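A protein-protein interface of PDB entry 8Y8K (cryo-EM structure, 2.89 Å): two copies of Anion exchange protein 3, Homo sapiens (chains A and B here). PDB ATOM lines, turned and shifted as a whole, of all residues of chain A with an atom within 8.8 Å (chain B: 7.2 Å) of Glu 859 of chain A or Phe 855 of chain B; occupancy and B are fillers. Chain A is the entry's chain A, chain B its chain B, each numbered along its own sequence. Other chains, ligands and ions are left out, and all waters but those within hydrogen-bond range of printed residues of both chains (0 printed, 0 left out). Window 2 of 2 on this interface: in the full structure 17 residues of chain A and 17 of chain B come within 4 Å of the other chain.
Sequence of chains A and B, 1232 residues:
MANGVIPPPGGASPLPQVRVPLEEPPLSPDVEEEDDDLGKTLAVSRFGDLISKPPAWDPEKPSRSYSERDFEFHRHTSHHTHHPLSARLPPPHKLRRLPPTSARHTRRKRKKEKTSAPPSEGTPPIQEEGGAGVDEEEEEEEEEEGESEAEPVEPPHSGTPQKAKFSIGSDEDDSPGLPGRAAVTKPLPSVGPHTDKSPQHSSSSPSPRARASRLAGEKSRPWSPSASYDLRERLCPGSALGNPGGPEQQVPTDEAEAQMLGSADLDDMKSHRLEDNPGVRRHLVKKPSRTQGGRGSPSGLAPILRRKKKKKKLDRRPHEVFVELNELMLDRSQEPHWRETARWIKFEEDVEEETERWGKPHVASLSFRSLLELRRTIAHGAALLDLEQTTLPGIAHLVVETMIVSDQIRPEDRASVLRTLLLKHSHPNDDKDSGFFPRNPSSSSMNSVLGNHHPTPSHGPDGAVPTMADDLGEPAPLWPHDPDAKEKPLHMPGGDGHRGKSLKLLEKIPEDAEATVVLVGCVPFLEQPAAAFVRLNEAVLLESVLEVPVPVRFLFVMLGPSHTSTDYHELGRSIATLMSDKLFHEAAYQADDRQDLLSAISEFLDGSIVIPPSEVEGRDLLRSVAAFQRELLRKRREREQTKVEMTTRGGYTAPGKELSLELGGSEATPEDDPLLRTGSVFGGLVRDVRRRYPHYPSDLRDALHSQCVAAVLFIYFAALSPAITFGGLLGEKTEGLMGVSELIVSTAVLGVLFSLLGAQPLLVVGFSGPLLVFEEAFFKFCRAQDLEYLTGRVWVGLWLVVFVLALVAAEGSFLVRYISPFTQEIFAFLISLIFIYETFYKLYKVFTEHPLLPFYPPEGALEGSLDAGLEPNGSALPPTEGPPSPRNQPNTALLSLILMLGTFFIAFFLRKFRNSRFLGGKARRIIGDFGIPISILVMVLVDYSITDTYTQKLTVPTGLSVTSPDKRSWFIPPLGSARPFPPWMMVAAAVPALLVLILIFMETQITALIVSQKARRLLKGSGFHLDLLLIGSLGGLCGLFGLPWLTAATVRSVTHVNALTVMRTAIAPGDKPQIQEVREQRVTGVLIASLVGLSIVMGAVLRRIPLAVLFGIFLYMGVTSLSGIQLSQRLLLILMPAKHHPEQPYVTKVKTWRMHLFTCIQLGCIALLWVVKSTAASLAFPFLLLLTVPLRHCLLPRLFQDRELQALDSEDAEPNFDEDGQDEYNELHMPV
CE1 of Phe 855 of chain B touches CA of Pro 858 of chain A (3.6 Å).
Glu 859 of chain A touches Phe 855 of chain B (N to CE1, 3.7 Å).
Leu 852 of chain B touches Asn 891 of chain A (CD2 to ND2, 3.8 Å).
Asn 891 of chain A touches Tyr 856 of chain B.
CA of Leu 853 of chain B touches OD1 of Asp 948 of chain A, at 3.8 Å.
Pro 854 of chain B touches Asp 948 of chain A.
The backbone carbonyl oxygen of Tyr 856 of chain A lies close to the backbone carbonyl oxygen of Tyr 856 of chain B (3.2 Å).
OD1 of Asp 948 of chain A sits close to O of Leu 852 of chain B (2.8 Å).
Of the 7 printed residues of chain B, 5 touch a printed residue of chain A.
Among the printed residues, 8 pairs touch across the chains.
Among the printed residues, no Asp or Glu carboxylate lies within 4 Å of a Lys or Arg side-chain nitrogen of the other chain.
N of Leu 853 of chain B is in hydrogen-bond range of OH of Tyr 856 of chain B, at 2.6 Å.
Phe 855 of chain B touches just these residues of chain A: Pro 858 and Glu 859.
Pro 854 of chain B touches one residue of chain A.
Printed residues of chain A within 4 Å of Leu 853 of chain B: Asp 948 (3.8 Å).
Printed residues of chain B within 4 Å of Tyr 856 of chain A: Tyr 856.
His 850 of chain A touches none of the printed residues of chain B.
Pro 886 of chain A touches none of the printed residues of chain B.
Tyr 856 of chain A touches its own counterpart, Tyr 856 of chain B.
Of the 8 pairs that touch across the chains among the printed residues, 1 has its exchanged pair printed and touching as well.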
ATOM      1  N   HIS A 850       5.806  -1.155  11.272  1.00  0.00           N
ATOM      2  CA  HIS A 850       7.162  -1.307  10.738  1.00  0.00           C
ATOM      3  C   HIS A 850       7.135  -1.223   9.218  1.00  0.00           C
ATOM      4  O   HIS A 850       7.233  -2.246   8.527  1.00  0.00           O
ATOM      5  CB  HIS A 850       7.774  -2.638  11.172  1.00  0.00           C
ATOM      6  CG  HIS A 850       7.928  -2.784  12.652  1.00  0.00           C
ATOM      7  ND1 HIS A 850       8.879  -2.097  13.373  1.00  0.00           N
ATOM      8  CD2 HIS A 850       7.256  -3.544  13.547  1.00  0.00           C
ATOM      9  CE1 HIS A 850       8.788  -2.428  14.647  1.00  0.00           C
ATOM     10  NE2 HIS A 850       7.809  -3.303  14.781  1.00  0.00           N
ATOM     11  N   TYR A 856      17.201   3.502   6.759  1.00  0.00           N
ATOM     12  CA  TYR A 856      16.901   3.202   8.158  1.00  0.00           C
ATOM     13  C   TYR A 856      18.022   3.775   9.014  1.00  0.00           C
ATOM     14  O   TYR A 856      19.020   3.091   9.290  1.00  0.00           O
ATOM     15  CB  TYR A 856      16.743   1.700   8.374  1.00  0.00           C
ATOM     16  CG  TYR A 856      15.435   1.175   7.844  1.00  0.00           C
ATOM     17  CD1 TYR A 856      14.255   1.364   8.545  1.00  0.00           C
ATOM     18  CD2 TYR A 856      15.373   0.518   6.627  1.00  0.00           C
ATOM     19  CE1 TYR A 856      13.055   0.897   8.057  1.00  0.00           C
ATOM     20  CE2 TYR A 856      14.179   0.049   6.131  1.00  0.00           C
ATOM     21  CZ  TYR A 856      13.024   0.240   6.850  1.00  0.00           C
ATOM     22  OH  TYR A 856      11.830  -0.229   6.357  1.00  0.00           O
ATOM     23  N   PRO A 857      17.900   5.028   9.455  1.00  0.00           N
ATOM     24  CA  PRO A 857      18.999   5.648  10.189  1.00  0.00           C
ATOM     25  C   PRO A 857      19.151   5.029  11.560  1.00  0.00           C
ATOM     26  O   PRO A 857      18.166   4.572  12.168  1.00  0.00           O
ATOM     27  CB  PRO A 857      18.577   7.128  10.279  1.00  0.00           C
ATOM     28  CG  PRO A 857      17.150   7.199   9.807  1.00  0.00           C
ATOM     29  CD  PRO A 857      16.666   5.826   9.497  1.00  0.00           C
ATOM     30  N   PRO A 858      20.369   4.983  12.099  1.00  0.00           N
ATOM     31  CA  PRO A 858      20.570   4.396  13.427  1.00  0.00           C
ATOM     32  C   PRO A 858      19.875   5.203  14.512  1.00  0.00           C
ATOM     33  O   PRO A 858      19.723   6.423  14.415  1.00  0.00           O
ATOM     34  CB  PRO A 858      22.092   4.423  13.602  1.00  0.00           C
ATOM     35  CG  PRO A 858      22.554   5.519  12.700  1.00  0.00           C
ATOM     36  CD  PRO A 858      21.624   5.494  11.521  1.00  0.00           C
ATOM     37  N   GLU A 859      19.450   4.498  15.556  1.00  0.00           N
ATOM     38  CA  GLU A 859      18.739   5.111  16.671  1.00  0.00           C
ATOM     39  C   GLU A 859      19.632   6.088  17.430  1.00  0.00           C
ATOM     40  O   GLU A 859      19.316   7.272  17.545  1.00  0.00           O
ATOM     41  CB  GLU A 859      18.210   4.036  17.625  1.00  0.00           C
ATOM     42  CG  GLU A 859      17.219   3.070  16.989  1.00  0.00           C
ATOM     43  CD  GLU A 859      15.882   3.718  16.685  1.00  0.00           C
ATOM     44  OE1 GLU A 859      15.462   4.608  17.455  1.00  0.00           O
ATOM     45  OE2 GLU A 859      15.251   3.339  15.676  1.00  0.00           O
ATOM     46  N   SER A 885       8.366   0.147  22.999  1.00  0.00           N
ATOM     47  CA  SER A 885       8.447  -0.893  21.986  1.00  0.00           C
ATOM     48  C   SER A 885       9.158  -0.363  20.742  1.00  0.00           C
ATOM     49  O   SER A 885       9.004   0.811  20.393  1.00  0.00           O
ATOM     50  CB  SER A 885       7.051  -1.390  21.614  1.00  0.00           C
ATOM     51  OG  SER A 885       6.291  -0.359  21.010  1.00  0.00           O
ATOM     52  N   PRO A 886       9.945  -1.195  20.063  1.00  0.00           N
ATOM     53  CA  PRO A 886      10.616  -0.742  18.840  1.00  0.00           C
ATOM     54  C   PRO A 886       9.622  -0.369  17.750  1.00  0.00           C
ATOM     55  O   PRO A 886       8.558  -0.973  17.612  1.00  0.00           O
ATOM     56  CB  PRO A 886      11.464  -1.953  18.432  1.00  0.00           C
ATOM     57  CG  PRO A 886      11.638  -2.733  19.691  1.00  0.00           C
ATOM     58  CD  PRO A 886      10.365  -2.551  20.452  1.00  0.00           C
ATOM     59  N   ARG A 887       9.988   0.649  16.975  1.00  0.00           N
ATOM     60  CA  ARG A 887       9.192   1.098  15.843  1.00  0.00           C
ATOM     61  C   ARG A 887      10.119   1.432  14.684  1.00  0.00           C
ATOM     62  O   ARG A 887      11.274   1.813  14.888  1.00  0.00           O
ATOM     63  CB  ARG A 887       8.334   2.317  16.202  1.00  0.00           C
ATOM     64  CG  ARG A 887       6.861   2.006  16.392  1.00  0.00           C
ATOM     65  CD  ARG A 887       6.030   3.276  16.434  1.00  0.00           C
ATOM     66  NE  ARG A 887       4.642   3.036  16.057  1.00  0.00           N
ATOM     67  CZ  ARG A 887       4.095   3.436  14.916  1.00  0.00           C
ATOM     68  NH1 ARG A 887       4.796   4.095  14.007  1.00  0.00           N
ATOM     69  NH2 ARG A 887       2.814   3.167  14.680  1.00  0.00           N
ATOM     70  N   ASN A 888       9.598   1.281  13.465  1.00  0.00           N
ATOM     71  CA  ASN A 888      10.344   1.544  12.234  1.00  0.00           C
ATOM     72  C   ASN A 888      11.613   0.692  12.165  1.00  0.00           C
ATOM     73  O   ASN A 888      12.735   1.199  12.108  1.00  0.00           O
ATOM     74  CB  ASN A 888      10.673   3.034  12.101  1.00  0.00           C
ATOM     75  CG  ASN A 888       9.454   3.877  11.793  1.00  0.00           C
ATOM     76  OD1 ASN A 888       8.630   3.512  10.959  1.00  0.00           O
ATOM     77  ND2 ASN A 888       9.334   5.012  12.468  1.00  0.00           N
ATOM     78  N   GLN A 889      11.416  -0.629  12.166  1.00  0.00           N
ATOM     79  CA  GLN A 889      12.509  -1.587  12.110  1.00  0.00           C
ATOM     80  C   GLN A 889      12.599  -2.233  10.729  1.00  0.00           C
ATOM     81  O   GLN A 889      11.587  -2.378  10.037  1.00  0.00           O
ATOM     82  CB  GLN A 889      12.335  -2.683  13.166  1.00  0.00           C
ATOM     83  CG  GLN A 889      12.385  -2.184  14.594  1.00  0.00           C
ATOM     84  CD  GLN A 889      13.799  -1.944  15.081  1.00  0.00           C
ATOM     85  OE1 GLN A 889      14.704  -2.727  14.801  1.00  0.00           O
ATOM     86  NE2 GLN A 889      13.997  -0.854  15.810  1.00  0.00           N
ATOM     87  N   PRO A 890      13.797  -2.616  10.294  1.00  0.00           N
ATOM     88  CA  PRO A 890      13.934  -3.299   9.005  1.00  0.00           C
ATOM     89  C   PRO A 890      13.770  -4.808   9.123  1.00  0.00           C
ATOM     90  O   PRO A 890      14.088  -5.419  10.145  1.00  0.00           O
ATOM     91  CB  PRO A 890      15.358  -2.937   8.572  1.00  0.00           C
ATOM     92  CG  PRO A 890      16.089  -2.761   9.851  1.00  0.00           C
ATOM     93  CD  PRO A 890      15.103  -2.206  10.842  1.00  0.00           C
ATOM     94  N   ASN A 891      13.255  -5.399   8.042  1.00  0.00           N
ATOM     95  CA  ASN A 891      13.096  -6.845   7.879  1.00  0.00           C
ATOM     96  C   ASN A 891      12.146  -7.463   8.901  1.00  0.00           C
ATOM     97  O   ASN A 891      12.250  -8.655   9.201  1.00  0.00           O
ATOM     98  CB  ASN A 891      14.449  -7.565   7.936  1.00  0.00           C
ATOM     99  CG  ASN A 891      15.487  -6.929   7.043  1.00  0.00           C
ATOM    100  OD1 ASN A 891      15.197  -6.546   5.914  1.00  0.00           O
ATOM    101  ND2 ASN A 891      16.706  -6.813   7.545  1.00  0.00           N
ATOM    102  N   ASP A 948      19.202 -11.751  14.258  1.00  0.00           N
ATOM    103  CA  ASP A 948      19.608 -10.388  13.939  1.00  0.00           C
ATOM    104  C   ASP A 948      18.449  -9.406  13.905  1.00  0.00           C
ATOM    105  O   ASP A 948      18.680  -8.203  14.060  1.00  0.00           O
ATOM    106  CB  ASP A 948      20.341 -10.342  12.594  1.00  0.00           C
ATOM    107  CG  ASP A 948      21.646  -9.578  12.675  1.00  0.00           C
ATOM    108  OD1 ASP A 948      22.429  -9.625  11.703  1.00  0.00           O
ATOM    109  OD2 ASP A 948      21.894  -8.948  13.721  1.00  0.00           O
ATOM    110  N   THR A 949      17.218  -9.873  13.713  1.00  0.00           N
ATOM    111  CA  THR A 949      16.062  -9.037  13.426  1.00  0.00           C
ATOM    112  C   THR A 949      15.103  -9.042  14.609  1.00  0.00           C
ATOM    113  O   THR A 949      15.085  -9.986  15.404  1.00  0.00           O
ATOM    114  CB  THR A 949      15.343  -9.539  12.170  1.00  0.00           C
ATOM    115  OG1 THR A 949      16.313  -9.955  11.202  1.00  0.00           O
ATOM    116  CG2 THR A 949      14.483  -8.454  11.563  1.00  0.00           C
ATOM    117  N   LEU B 852      20.909  -9.895   6.147  1.00  0.00           N
ATOM    118  CA  LEU B 852      20.010  -9.287   7.123  1.00  0.00           C
ATOM    119  C   LEU B 852      20.851  -8.736   8.269  1.00  0.00           C
ATOM    120  O   LEU B 852      21.360  -9.496   9.097  1.00  0.00           O
ATOM    121  CB  LEU B 852      18.987 -10.300   7.631  1.00  0.00           C
ATOM    122  CG  LEU B 852      18.037 -10.965   6.629  1.00  0.00           C
ATOM    123  CD1 LEU B 852      16.875 -11.609   7.358  1.00  0.00           C
ATOM    124  CD2 LEU B 852      17.532  -9.978   5.595  1.00  0.00           C
ATOM    125  N   LEU B 853      20.995  -7.411   8.317  1.00  0.00           N
ATOM    126  CA  LEU B 853      21.850  -6.720   9.269  1.00  0.00           C
ATOM    127  C   LEU B 853      21.013  -6.008  10.329  1.00  0.00           C
ATOM    128  O   LEU B 853      19.844  -5.689  10.089  1.00  0.00           O
ATOM    129  CB  LEU B 853      22.738  -5.694   8.552  1.00  0.00           C
ATOM    130  CG  LEU B 853      23.714  -6.230   7.507  1.00  0.00           C
ATOM    131  CD1 LEU B 853      24.370  -5.083   6.763  1.00  0.00           C
ATOM    132  CD2 LEU B 853      24.756  -7.125   8.151  1.00  0.00           C
ATOM    133  N   PRO B 854      21.573  -5.744  11.519  1.00  0.00           N
ATOM    134  CA  PRO B 854      20.810  -5.009  12.533  1.00  0.00           C
ATOM    135  C   PRO B 854      20.692  -3.533  12.196  1.00  0.00           C
ATOM    136  O   PRO B 854      19.630  -2.928  12.371  1.00  0.00           O
ATOM    137  CB  PRO B 854      21.620  -5.227  13.821  1.00  0.00           C
ATOM    138  CG  PRO B 854      22.843  -6.022  13.423  1.00  0.00           C
ATOM    139  CD  PRO B 854      22.967  -5.945  11.944  1.00  0.00           C
ATOM    140  N   PHE B 855      21.783  -2.951  11.705  1.00  0.00           N
ATOM    141  CA  PHE B 855      21.841  -1.542  11.359  1.00  0.00           C
ATOM    142  C   PHE B 855      22.229  -1.391   9.896  1.00  0.00           C
ATOM    143  O   PHE B 855      23.105  -2.100   9.393  1.00  0.00           O
ATOM    144  CB  PHE B 855      22.845  -0.796  12.244  1.00  0.00           C
ATOM    145  CG  PHE B 855      22.280  -0.359  13.560  1.00  0.00           C
ATOM    146  CD1 PHE B 855      21.479   0.765  13.646  1.00  0.00           C
ATOM    147  CD2 PHE B 855      22.549  -1.074  14.715  1.00  0.00           C
ATOM    148  CE1 PHE B 855      20.954   1.167  14.858  1.00  0.00           C
ATOM    149  CE2 PHE B 855      22.029  -0.676  15.930  1.00  0.00           C
ATOM    150  CZ  PHE B 855      21.230   0.446  16.002  1.00  0.00           C
ATOM    151  N   TYR B 856      21.573  -0.454   9.216  1.00  0.00           N
ATOM    152  CA  TYR B 856      21.772  -0.217   7.787  1.00  0.00           C
ATOM    153  C   TYR B 856      22.151   1.244   7.606  1.00  0.00           C
ATOM    154  O   TYR B 856      21.315   2.079   7.234  1.00  0.00           O
ATOM    155  CB  TYR B 856      20.521  -0.582   6.988  1.00  0.00           C
ATOM    156  CG  TYR B 856      20.369  -2.069   6.792  1.00  0.00           C
ATOM    157  CD1 TYR B 856      21.172  -2.755   5.895  1.00  0.00           C
ATOM    158  CD2 TYR B 856      19.448  -2.793   7.530  1.00  0.00           C
ATOM    159  CE1 TYR B 856      21.046  -4.117   5.724  1.00  0.00           C
ATOM    160  CE2 TYR B 856      19.316  -4.153   7.367  1.00  0.00           C
ATOM    161  CZ  TYR B 856      20.116  -4.809   6.463  1.00  0.00           C
ATOM    162  OH  TYR B 856      19.985  -6.167   6.297  1.00  0.00           O
ATOM    163  N   PRO B 857      23.411   1.587   7.854  1.00  0.00           N
ATOM    164  CA  PRO B 857      23.820   2.987   7.812  1.00  0.00           C
ATOM    165  C   PRO B 857      23.973   3.466   6.382  1.00  0.00           C
ATOM    166  O   PRO B 857      24.582   2.777   5.548  1.00  0.00           O
ATOM    167  CB  PRO B 857      25.167   2.990   8.553  1.00  0.00           C
ATOM    168  CG  PRO B 857      25.584   1.537   8.677  1.00  0.00           C
ATOM    169  CD  PRO B 857      24.557   0.678   8.007  1.00  0.00           C
ATOM    170  N   ASN B 888      24.376  -4.793   0.321  1.00  0.00           N
ATOM    171  CA  ASN B 888      23.943  -4.541   1.696  1.00  0.00           C
ATOM    172  C   ASN B 888      22.722  -3.622   1.736  1.00  0.00           C
ATOM    173  O   ASN B 888      22.749  -2.542   2.326  1.00  0.00           O
ATOM    174  CB  ASN B 888      25.087  -3.968   2.536  1.00  0.00           C
ATOM    175  CG  ASN B 888      26.208  -4.964   2.753  1.00  0.00           C
ATOM    176  OD1 ASN B 888      25.966  -6.135   3.032  1.00  0.00           O
ATOM    177  ND2 ASN B 888      27.443  -4.501   2.624  1.00  0.00           N
